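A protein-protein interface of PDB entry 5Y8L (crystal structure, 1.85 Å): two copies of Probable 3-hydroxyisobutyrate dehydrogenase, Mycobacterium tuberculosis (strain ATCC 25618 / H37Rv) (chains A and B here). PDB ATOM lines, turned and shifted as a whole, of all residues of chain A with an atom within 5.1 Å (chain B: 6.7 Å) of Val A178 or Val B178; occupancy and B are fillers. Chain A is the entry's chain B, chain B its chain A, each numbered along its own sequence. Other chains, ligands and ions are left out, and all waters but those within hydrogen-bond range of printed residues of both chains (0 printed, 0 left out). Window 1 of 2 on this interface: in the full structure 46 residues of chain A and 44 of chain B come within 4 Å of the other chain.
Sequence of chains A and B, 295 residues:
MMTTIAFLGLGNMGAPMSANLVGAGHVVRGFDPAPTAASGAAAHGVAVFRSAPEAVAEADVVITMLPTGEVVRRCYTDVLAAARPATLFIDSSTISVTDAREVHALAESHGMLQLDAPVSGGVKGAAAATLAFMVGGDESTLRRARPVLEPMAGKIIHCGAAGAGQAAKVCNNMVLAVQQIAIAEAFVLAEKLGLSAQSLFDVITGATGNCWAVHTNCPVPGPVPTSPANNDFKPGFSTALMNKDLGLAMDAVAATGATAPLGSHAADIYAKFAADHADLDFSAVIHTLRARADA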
ATOM      1  N   MET A 174      21.989  11.657 -13.415  1.00  0.00           N
ATOM      2  CA  MET A 174      20.797  10.820 -13.206  1.00  0.00           C
ATOM      3  C   MET A 174      19.810  10.935 -14.391  1.00  0.00           C
ATOM      4  O   MET A 174      19.367   9.919 -14.978  1.00  0.00           O
ATOM      5  CB  MET A 174      20.080  11.217 -11.887  1.00  0.00           C
ATOM      6  CG  MET A 174      19.000  10.197 -11.500  1.00  0.00           C
ATOM      7  SD  MET A 174      18.294  10.568  -9.872  1.00  0.00           S
ATOM      8  CE  MET A 174      17.411  12.113 -10.149  1.00  0.00           C
ATOM      9  N   VAL A 175      19.519  12.151 -14.758  1.00  0.00           N
ATOM     10  CA  VAL A 175      18.686  12.436 -15.944  1.00  0.00           C
ATOM     11  C   VAL A 175      19.290  11.798 -17.209  1.00  0.00           C
ATOM     12  O   VAL A 175      18.573  11.100 -17.923  1.00  0.00           O
ATOM     13  CB  VAL A 175      18.498  13.923 -16.157  1.00  0.00           C
ATOM     14  CG1 VAL A 175      17.823  14.200 -17.511  1.00  0.00           C
ATOM     15  CG2 VAL A 175      17.688  14.457 -15.030  1.00  0.00           C
ATOM     16  N   LEU A 176      20.607  11.943 -17.408  1.00  0.00           N
ATOM     17  CA  LEU A 176      21.285  11.373 -18.523  1.00  0.00           C
ATOM     18  C   LEU A 176      21.168   9.866 -18.605  1.00  0.00           C
ATOM     19  O   LEU A 176      20.868   9.330 -19.658  1.00  0.00           O
ATOM     20  CB  LEU A 176      22.755  11.762 -18.520  1.00  0.00           C
ATOM     21  CG  LEU A 176      23.574  11.123 -19.653  1.00  0.00           C
ATOM     22  CD1 LEU A 176      23.083  11.580 -20.999  1.00  0.00           C
ATOM     23  CD2 LEU A 176      25.022  11.518 -19.397  1.00  0.00           C
ATOM     24  N   ALA A 177      21.296   9.180 -17.463  1.00  0.00           N
ATOM     25  CA  ALA A 177      21.167   7.743 -17.415  1.00  0.00           C
ATOM     26  C   ALA A 177      19.763   7.283 -17.799  1.00  0.00           C
ATOM     27  O   ALA A 177      19.617   6.326 -18.588  1.00  0.00           O
ATOM     28  CB  ALA A 177      21.542   7.214 -16.012  1.00  0.00           C
ATOM     29  N   VAL A 178      18.759   7.948 -17.242  1.00  0.00           N
ATOM     30  CA  VAL A 178      17.368   7.708 -17.596  1.00  0.00           C
ATOM     31  C   VAL A 178      17.140   7.898 -19.097  1.00  0.00           C
ATOM     32  O   VAL A 178      16.604   6.992 -19.769  1.00  0.00           O
ATOM     33  CB  VAL A 178      16.450   8.618 -16.772  1.00  0.00           C
ATOM     34  CG1 VAL A 178      15.014   8.563 -17.283  1.00  0.00           C
ATOM     35  CG2 VAL A 178      16.484   8.226 -15.300  1.00  0.00           C
ATOM     36  N   GLN A 179      17.668   8.973 -19.653  1.00  0.00           N
ATOM     37  CA  GLN A 179      17.499   9.268 -21.113  1.00  0.00           C
ATOM     38  C   GLN A 179      18.184   8.240 -21.964  1.00  0.00           C
ATOM     39  O   GLN A 179      17.659   7.871 -23.002  1.00  0.00           O
ATOM     40  CB  GLN A 179      18.081  10.630 -21.486  1.00  0.00           C
ATOM     41  CG  GLN A 179      17.249  11.774 -20.934  1.00  0.00           C
ATOM     42  CD  GLN A 179      17.982  13.118 -20.883  1.00  0.00           C
ATOM     43  OE1 GLN A 179      19.223  13.173 -20.848  1.00  0.00           O
ATOM     44  NE2 GLN A 179      17.220  14.196 -20.823  1.00  0.00           N
ATOM     45  N   GLN A 180      19.361   7.813 -21.562  1.00  0.00           N
ATOM     46  CA  GLN A 180      20.115   6.831 -22.389  1.00  0.00           C
ATOM     47  C   GLN A 180      19.397   5.486 -22.473  1.00  0.00           C
ATOM     48  O   GLN A 180      19.373   4.794 -23.534  1.00  0.00           O
ATOM     49  CB  GLN A 180      21.544   6.643 -21.874  1.00  0.00           C
ATOM     50  CG  GLN A 180      22.451   5.918 -22.827  1.00  0.00           C
ATOM     51  CD  GLN A 180      22.790   6.718 -24.083  1.00  0.00           C
ATOM     52  OE1 GLN A 180      23.452   7.752 -24.009  1.00  0.00           O
ATOM     53  NE2 GLN A 180      22.211   6.326 -25.191  1.00  0.00           N
ATOM     54  N   ILE A 181      18.841   5.076 -21.370  1.00  0.00           N
ATOM     55  CA  ILE A 181      18.026   3.824 -21.358  1.00  0.00           C
ATOM     56  C   ILE A 181      16.749   4.029 -22.198  1.00  0.00           C
ATOM     57  O   ILE A 181      16.393   3.147 -23.006  1.00  0.00           O
ATOM     58  CB  ILE A 181      17.646   3.445 -19.926  1.00  0.00           C
ATOM     59  CG1 ILE A 181      18.906   2.988 -19.170  1.00  0.00           C
ATOM     60  CG2 ILE A 181      16.636   2.338 -19.895  1.00  0.00           C
ATOM     61  CD1 ILE A 181      18.763   2.933 -17.661  1.00  0.00           C
ATOM     62  N   ALA A 182      16.036   5.154 -21.977  1.00  0.00           N
ATOM     63  CA  ALA A 182      14.792   5.446 -22.720  1.00  0.00           C
ATOM     64  C   ALA A 182      14.988   5.468 -24.203  1.00  0.00           C
ATOM     65  O   ALA A 182      14.170   4.924 -24.918  1.00  0.00           O
ATOM     66  CB  ALA A 182      14.148   6.716 -22.256  1.00  0.00           C
ATOM     67  N   ILE A 183      16.066   6.101 -24.655  1.00  0.00           N
ATOM     68  CA  ILE A 183      16.415   6.149 -26.039  1.00  0.00           C
ATOM     69  C   ILE A 183      16.696   4.754 -26.552  1.00  0.00           C
ATOM     70  O   ILE A 183      16.255   4.413 -27.658  1.00  0.00           O
ATOM     71  CB  ILE A 183      17.578   7.103 -26.321  1.00  0.00           C
ATOM     72  CG1 ILE A 183      17.108   8.593 -26.123  1.00  0.00           C
ATOM     73  CG2 ILE A 183      18.215   6.841 -27.696  1.00  0.00           C
ATOM     74  CD1 ILE A 183      16.037   9.086 -27.068  1.00  0.00           C
ATOM     75  N   LEU A 262      12.267   6.774 -11.511  1.00  0.00           N
ATOM     76  CA  LEU A 262      12.949   6.374 -12.738  1.00  0.00           C
ATOM     77  C   LEU A 262      14.447   6.432 -12.539  1.00  0.00           C
ATOM     78  O   LEU A 262      15.146   5.584 -13.045  1.00  0.00           O
ATOM     79  CB  LEU A 262      12.551   7.229 -13.954  1.00  0.00           C
ATOM     80  CG  LEU A 262      11.009   7.160 -14.241  1.00  0.00           C
ATOM     81  CD1 LEU A 262      10.694   7.830 -15.576  1.00  0.00           C
ATOM     82  CD2 LEU A 262      10.416   5.765 -14.279  1.00  0.00           C
ATOM     83  N   GLY A 263      14.938   7.449 -11.804  1.00  0.00           N
ATOM     84  CA  GLY A 263      16.382   7.567 -11.524  1.00  0.00           C
ATOM     85  C   GLY A 263      16.857   6.336 -10.741  1.00  0.00           C
ATOM     86  O   GLY A 263      17.868   5.771 -11.077  1.00  0.00           O
ATOM     87  N   ALA A 266      16.771   3.358 -13.165  1.00  0.00           N
ATOM     88  CA  ALA A 266      17.969   3.428 -13.930  1.00  0.00           C
ATOM     89  C   ALA A 266      19.256   2.975 -13.187  1.00  0.00           C
ATOM     90  O   ALA A 266      20.143   2.328 -13.776  1.00  0.00           O
ATOM     91  CB  ALA A 266      18.157   4.789 -14.555  1.00  0.00           C
ATOM     92  N   ASN B 173       6.936   9.814 -28.035  1.00  0.00           N
ATOM     93  CA  ASN B 173       6.206  10.204 -26.857  1.00  0.00           C
ATOM     94  C   ASN B 173       6.504   9.366 -25.609  1.00  0.00           C
ATOM     95  O   ASN B 173       6.349   9.875 -24.486  1.00  0.00           O
ATOM     96  CB  ASN B 173       4.694  10.326 -27.115  1.00  0.00           C
ATOM     97  CG  ASN B 173       4.351  11.610 -27.885  1.00  0.00           C
ATOM     98  OD1 ASN B 173       5.251  12.275 -28.475  1.00  0.00           O
ATOM     99  ND2 ASN B 173       3.059  11.968 -27.920  1.00  0.00           N
ATOM    100  N   MET B 174       6.849   8.093 -25.813  1.00  0.00           N
ATOM    101  CA  MET B 174       7.270   7.245 -24.669  1.00  0.00           C
ATOM    102  C   MET B 174       8.565   7.869 -24.039  1.00  0.00           C
ATOM    103  O   MET B 174       8.670   7.977 -22.829  1.00  0.00           O
ATOM    104  CB  MET B 174       7.539   5.824 -25.106  1.00  0.00           C
ATOM    105  CG  MET B 174       7.880   4.857 -23.985  1.00  0.00           C
ATOM    106  SD  MET B 174       8.061   3.153 -24.551  1.00  0.00           S
ATOM    107  CE  MET B 174       9.466   3.153 -25.644  1.00  0.00           C
ATOM    108  N   VAL B 175       9.511   8.270 -24.880  1.00  0.00           N
ATOM    109  CA  VAL B 175      10.748   8.908 -24.438  1.00  0.00           C
ATOM    110  C   VAL B 175      10.404  10.222 -23.705  1.00  0.00           C
ATOM    111  O   VAL B 175      10.983  10.519 -22.648  1.00  0.00           O
ATOM    112  CB  VAL B 175      11.705   9.189 -25.619  1.00  0.00           C
ATOM    113  CG1 VAL B 175      12.879  10.112 -25.231  1.00  0.00           C
ATOM    114  CG2 VAL B 175      12.183   7.909 -26.239  1.00  0.00           C
ATOM    115  N   LEU B 176       9.503  11.011 -24.284  1.00  0.00           N
ATOM    116  CA  LEU B 176       9.116  12.299 -23.714  1.00  0.00           C
ATOM    117  C   LEU B 176       8.547  12.134 -22.302  1.00  0.00           C
ATOM    118  O   LEU B 176       8.858  12.893 -21.443  1.00  0.00           O
ATOM    119  CB  LEU B 176       8.090  12.969 -24.598  1.00  0.00           C
ATOM    120  CG  LEU B 176       7.563  14.310 -24.127  1.00  0.00           C
ATOM    121  CD1 LEU B 176       8.653  15.369 -24.010  1.00  0.00           C
ATOM    122  CD2 LEU B 176       6.465  14.753 -25.057  1.00  0.00           C
ATOM    123  N   ALA B 177       7.731  11.103 -22.116  1.00  0.00           N
ATOM    124  CA  ALA B 177       7.105  10.863 -20.829  1.00  0.00           C
ATOM    125  C   ALA B 177       8.173  10.547 -19.802  1.00  0.00           C
ATOM    126  O   ALA B 177       8.156  11.057 -18.683  1.00  0.00           O
ATOM    127  CB  ALA B 177       6.074   9.750 -20.944  1.00  0.00           C
ATOM    128  N   VAL B 178       9.104   9.677 -20.178  1.00  0.00           N
ATOM    129  CA  VAL B 178      10.229   9.292 -19.296  1.00  0.00           C
ATOM    130  C   VAL B 178      11.035  10.561 -18.962  1.00  0.00           C
ATOM    131  O   VAL B 178      11.357  10.826 -17.818  1.00  0.00           O
ATOM    132  CB  VAL B 178      11.142   8.224 -19.932  1.00  0.00           C
ATOM    133  CG1 VAL B 178      12.456   8.076 -19.172  1.00  0.00           C
ATOM    134  CG2 VAL B 178      10.452   6.894 -20.079  1.00  0.00           C
ATOM    135  N   GLN B 179      11.349  11.355 -19.971  1.00  0.00           N
ATOM    136  CA  GLN B 179      12.114  12.603 -19.754  1.00  0.00           C
ATOM    137  C   GLN B 179      11.385  13.595 -18.836  1.00  0.00           C
ATOM    138  O   GLN B 179      12.033  14.225 -17.982  1.00  0.00           O
ATOM    139  CB  GLN B 179      12.418  13.301 -21.062  1.00  0.00           C
ATOM    140  CG  GLN B 179      13.430  12.576 -21.936  1.00  0.00           C
ATOM    141  CD  GLN B 179      13.442  13.095 -23.381  1.00  0.00           C
ATOM    142  OE1 GLN B 179      12.446  13.639 -23.863  1.00  0.00           O
ATOM    143  NE2 GLN B 179      14.596  12.936 -24.084  1.00  0.00           N
ATOM    144  N   GLN B 180      10.050  13.749 -19.013  1.00  0.00           N
ATOM    145  CA  GLN B 180       9.330  14.694 -18.159  1.00  0.00           C
ATOM    146  C   GLN B 180       9.317  14.272 -16.699  1.00  0.00           C
ATOM    147  O   GLN B 180       9.461  15.121 -15.812  1.00  0.00           O
ATOM    148  CB  GLN B 180       7.892  14.930 -18.658  1.00  0.00           C
ATOM    149  CG  GLN B 180       7.242  16.161 -18.032  1.00  0.00           C
ATOM    150  CD  GLN B 180       7.808  17.464 -18.536  1.00  0.00           C
ATOM    151  OE1 GLN B 180       7.704  17.812 -19.680  1.00  0.00           O
ATOM    152  NE2 GLN B 180       8.457  18.172 -17.677  1.00  0.00           N
ATOM    153  N   ILE B 181       9.208  12.958 -16.441  1.00  0.00           N
ATOM    154  CA  ILE B 181       9.303  12.494 -15.083  1.00  0.00           C
ATOM    155  C   ILE B 181      10.753  12.638 -14.561  1.00  0.00           C
ATOM    156  O   ILE B 181      10.983  13.028 -13.434  1.00  0.00           O
ATOM    157  CB  ILE B 181       8.819  11.034 -14.970  1.00  0.00           C
ATOM    158  CG1 ILE B 181       7.309  10.945 -15.270  1.00  0.00           C
ATOM    159  CG2 ILE B 181       9.148  10.469 -13.580  1.00  0.00           C
ATOM    160  CD1 ILE B 181       6.881   9.581 -15.669  1.00  0.00           C
ATOM    161  N   ALA B 182      11.715  12.231 -15.365  1.00  0.00           N
ATOM    162  CA  ALA B 182      13.136  12.344 -14.944  1.00  0.00           C
ATOM    163  C   ALA B 182      13.549  13.796 -14.556  1.00  0.00           C
ATOM    164  O   ALA B 182      14.221  13.998 -13.531  1.00  0.00           O
ATOM    165  CB  ALA B 182      14.062  11.791 -16.005  1.00  0.00           C
ATOM    166  N   ILE B 183      13.098  14.784 -15.352  1.00  0.00           N
ATOM    167  CA  ILE B 183      13.339  16.198 -15.069  1.00  0.00           C
ATOM    168  C   ILE B 183      12.655  16.595 -13.756  1.00  0.00           C
ATOM    169  O   ILE B 183      13.259  17.354 -12.963  1.00  0.00           O
ATOM    170  CB  ILE B 183      12.856  17.082 -16.243  1.00  0.00           C
ATOM    171  CG1 ILE B 183      13.807  16.910 -17.479  1.00  0.00           C
ATOM    172  CG2 ILE B 183      12.780  18.514 -15.905  1.00  0.00           C
ATOM    173  CD1 ILE B 183      15.256  17.309 -17.315  1.00  0.00           C
ATOM    174  N   GLU B 185      11.989  14.616 -11.188  1.00  0.00           N
ATOM    175  CA  GLU B 185      12.790  14.024 -10.119  1.00  0.00           C
ATOM    176  C   GLU B 185      14.049  14.849  -9.849  1.00  0.00           C
ATOM    177  O   GLU B 185      14.395  15.072  -8.703  1.00  0.00           O
ATOM    178  CB  GLU B 185      13.236  12.621 -10.474  1.00  0.00           C
ATOM    179  CG  GLU B 185      12.096  11.643 -10.594  1.00  0.00           C
ATOM    180  CD  GLU B 185      12.545  10.256 -11.143  1.00  0.00           C
ATOM    181  OE1 GLU B 185      13.768   9.908 -11.294  1.00  0.00           O
ATOM    182  OE2 GLU B 185      11.620   9.486 -11.457  1.00  0.00           O
ATOM    183  N   MET B 242      -1.295  12.243 -22.617  1.00  0.00           N
ATOM    184  CA  MET B 242      -0.042  11.574 -22.424  1.00  0.00           C
ATOM    185  C   MET B 242      -0.331  10.121 -22.004  1.00  0.00           C
ATOM    186  O   MET B 242       0.285   9.190 -22.487  1.00  0.00           O
ATOM    187  CB  MET B 242       0.831  12.298 -21.380  1.00  0.00           C
ATOM    188  CG  MET B 242       2.104  11.532 -21.025  1.00  0.00           C
ATOM    189  SD  MET B 242       3.341  11.778 -22.342  1.00  0.00           S
ATOM    190  CE  MET B 242       3.092  10.490 -23.314  1.00  0.00           C
ATOM    191  N   LEU B 246       0.798   6.703 -23.976  1.00  0.00           N
ATOM    192  CA  LEU B 246       1.570   5.662 -23.334  1.00  0.00           C
ATOM    193  C   LEU B 246       0.825   4.338 -23.316  1.00  0.00           C
ATOM    194  O   LEU B 246       1.486   3.272 -23.347  1.00  0.00           O
ATOM    195  CB  LEU B 246       1.886   6.033 -21.895  1.00  0.00           C
ATOM    196  CG  LEU B 246       2.984   7.119 -21.824  1.00  0.00           C
ATOM    197  CD1 LEU B 246       3.084   7.792 -20.484  1.00  0.00           C
ATOM    198  CD2 LEU B 246       4.322   6.606 -22.258  1.00  0.00           C
ATOM    199  N   LEU B 262      11.754   1.457 -18.465  1.00  0.00           N
ATOM    200  CA  LEU B 262      11.464   2.793 -18.025  1.00  0.00           C
ATOM    201  C   LEU B 262      10.182   3.336 -18.688  1.00  0.00           C
ATOM    202  O   LEU B 262       9.356   3.972 -18.026  1.00  0.00           O
ATOM    203  CB  LEU B 262      12.642   3.753 -18.278  1.00  0.00           C
ATOM    204  CG  LEU B 262      13.913   3.362 -17.492  1.00  0.00           C
ATOM    205  CD1 LEU B 262      14.931   4.483 -17.620  1.00  0.00           C
ATOM    206  CD2 LEU B 262      13.681   3.004 -16.023  1.00  0.00           C
ATOM    207  N   GLY B 263      10.025   3.098 -19.995  1.00  0.00           N
ATOM    208  CA  GLY B 263       8.759   3.475 -20.617  1.00  0.00           C
ATOM    209  C   GLY B 263       7.549   2.847 -19.945  1.00  0.00           C
ATOM    210  O   GLY B 263       6.564   3.538 -19.700  1.00  0.00           O
ATOM    211  N   SER B 264       7.628   1.583 -19.570  1.00  0.00           N
ATOM    212  CA  SER B 264       6.508   0.939 -18.883  1.00  0.00           C
ATOM    213  C   SER B 264       6.265   1.474 -17.508  1.00  0.00           C
ATOM    214  O   SER B 264       5.124   1.574 -17.041  1.00  0.00           O
ATOM    215  CB  SER B 264       6.760  -0.565 -18.812  1.00  0.00           C
ATOM    216  OG  SER B 264       6.903  -1.074 -20.126  1.00  0.00           O
ATOM    217  N   HIS B 265       7.340   1.851 -16.830  1.00  0.00           N
ATOM    218  CA  HIS B 265       7.284   2.499 -15.537  1.00  0.00           C
ATOM    219  C   HIS B 265       6.616   3.896 -15.627  1.00  0.00           C
ATOM    220  O   HIS B 265       5.740   4.264 -14.836  1.00  0.00           O
ATOM    221  CB  HIS B 265       8.723   2.575 -14.920  1.00  0.00           C
ATOM    222  CG  HIS B 265       8.719   2.839 -13.434  1.00  0.00           C
ATOM    223  ND1 HIS B 265       9.804   2.569 -12.639  1.00  0.00           N
ATOM    224  CD2 HIS B 265       7.788   3.401 -12.618  1.00  0.00           C
ATOM    225  CE1 HIS B 265       9.559   2.960 -11.399  1.00  0.00           C
ATOM    226  NE2 HIS B 265       8.330   3.467 -11.357  1.00  0.00           N
ATOM    227  N   ALA B 266       7.024   4.659 -16.629  1.00  0.00           N
ATOM    228  CA  ALA B 266       6.407   5.951 -16.906  1.00  0.00           C
ATOM    229  C   ALA B 266       4.896   5.847 -17.207  1.00  0.00           C
ATOM    230  O   ALA B 266       4.113   6.640 -16.733  1.00  0.00           O
ATOM    231  CB  ALA B 266       7.108   6.606 -18.094  1.00  0.00           C
ATOM    232  N   ALA B 267       4.540   4.832 -17.974  1.00  0.00           N
ATOM    233  CA  ALA B 267       3.157   4.505 -18.298  1.00  0.00           C
ATOM    234  C   ALA B 267       2.419   4.256 -16.988  1.00  0.00           C
ATOM    235  O   ALA B 267       1.335   4.857 -16.759  1.00  0.00           O
ATOM    236  CB  ALA B 267       3.089   3.315 -19.239  1.00  0.00           C
ATOM    237  N   TYR B 270       1.958   7.571 -15.202  1.00  0.00           N
ATOM    238  CA  TYR B 270       1.024   8.537 -15.755  1.00  0.00           C
ATOM    239  C   TYR B 270      -0.449   7.994 -15.629  1.00  0.00           C
ATOM    240  O   TYR B 270      -1.333   8.818 -15.531  1.00  0.00           O
ATOM    241  CB  TYR B 270       1.376   8.949 -17.197  1.00  0.00           C
ATOM    242  CG  TYR B 270       2.331  10.152 -17.201  1.00  0.00           C
ATOM    243  CD1 TYR B 270       1.890  11.379 -16.762  1.00  0.00           C
ATOM    244  CD2 TYR B 270       3.663  10.033 -17.608  1.00  0.00           C
ATOM    245  CE1 TYR B 270       2.712  12.505 -16.731  1.00  0.00           C
ATOM    246  CE2 TYR B 270       4.519  11.170 -17.636  1.00  0.00           C
ATOM    247  CZ  TYR B 270       4.051  12.402 -17.168  1.00  0.00           C
ATOM    248  OH  TYR B 270       4.795  13.580 -17.133  1.00  0.00           O
ATOM    249  N   PHE B 282       0.977  17.420 -18.416  1.00  0.00           N
ATOM    250  CA  PHE B 282       1.796  16.320 -17.949  1.00  0.00           C
ATOM    251  C   PHE B 282       3.016  16.635 -17.093  1.00  0.00           C
ATOM    252  O   PHE B 282       3.472  15.749 -16.379  1.00  0.00           O
ATOM    253  CB  PHE B 282       2.078  15.332 -19.058  1.00  0.00           C
ATOM    254  CG  PHE B 282       3.238  15.672 -19.945  1.00  0.00           C
ATOM    255  CD1 PHE B 282       3.281  16.858 -20.633  1.00  0.00           C
ATOM    256  CD2 PHE B 282       4.240  14.766 -20.123  1.00  0.00           C
ATOM    257  CE1 PHE B 282       4.359  17.168 -21.441  1.00  0.00           C
ATOM    258  CE2 PHE B 282       5.302  15.047 -20.975  1.00  0.00           C
ATOM    259  CZ  PHE B 282       5.342  16.262 -21.626  1.00  0.00           C
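OE1 of Glu B185 lies within hydrogen-bond range of N of Gly A263 (2.8 Å). OE2 of Glu B185 lies within hydrogen-bond range of N of Leu A262, 2.8 Å away.
Ala A177 touches none of the printed residues of chain B. Of the printed residues of chain B, Ile A181 touches Leu B262 (3.6 Å). Printed residues of chain B within 4 Å of Ala A182: Val B175 (3.8 Å) and Val B178 (3.8 Å). Printed residues of chain A within 4 Å of Val B178: Val A178, Ala A182 and Leu A262. Printed residues of chain A within 4 Å of Ile B181: Leu A262. Of the printed residues of chain A, Glu B185 touches Leu A262 and Gly A263. Of the printed residues of chain A, Leu B262 touches Val A178 and Ile A181. The nearest residue of chain B that does not touch Val A178 is Glu B185 (5.1 Å).
Val B178 touches its own counterpart, Val A178. Val A178 touches Ala B182, and with the chains exchanged Ala A182 touches Val B178. Val A178 touches Leu B262, and with the chains exchanged Leu A262 touches Val B178. Ile A181 touches Leu B262, and with the chains exchanged Leu A262 touches Ile B181. Of the 13 pairs that touch across the chains among the printed residues, 9 have their exchanged pair printed and touching as well.
Among the printed residues, merely in contact across the chains: Val A178 with Val B178, Leu A262 with His B265, Ile A181 with Leu B262, Val A178 with Ala B182, Leu A262 with Ile B181, Val A178 with Leu B262, Ala A182 with Val B178, Ile A183 with Val B175, Leu A262 with Val B178, Val A175 with Ala B182 and Ala A182 with Val B175.
Hydrophobic or aromatic side chains of chain B that line the printed part of chain A: Val B175, Val B178, Ile B181, Ala B182, Leu B262 and His B265. Of the 13 printed residues of chain A, 7 touch a printed residue of chain B. Printed residues of chain A that touch a printed residue of chain B: Val A175, Val A178, Ile A181, Ala A182, Ile A183, Leu A262 and Gly A263. Hydrophobic or aromatic side chains of chain A within 4 Å of the printed part of chain B: Val A175, Val A178, Ile A181, Ala A182, Ile A183 and Leu A262. Among the printed residues, no Asp or Glu carboxylate lies within 4 Å of a Lys or Arg side-chain nitrogen of the other chain.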
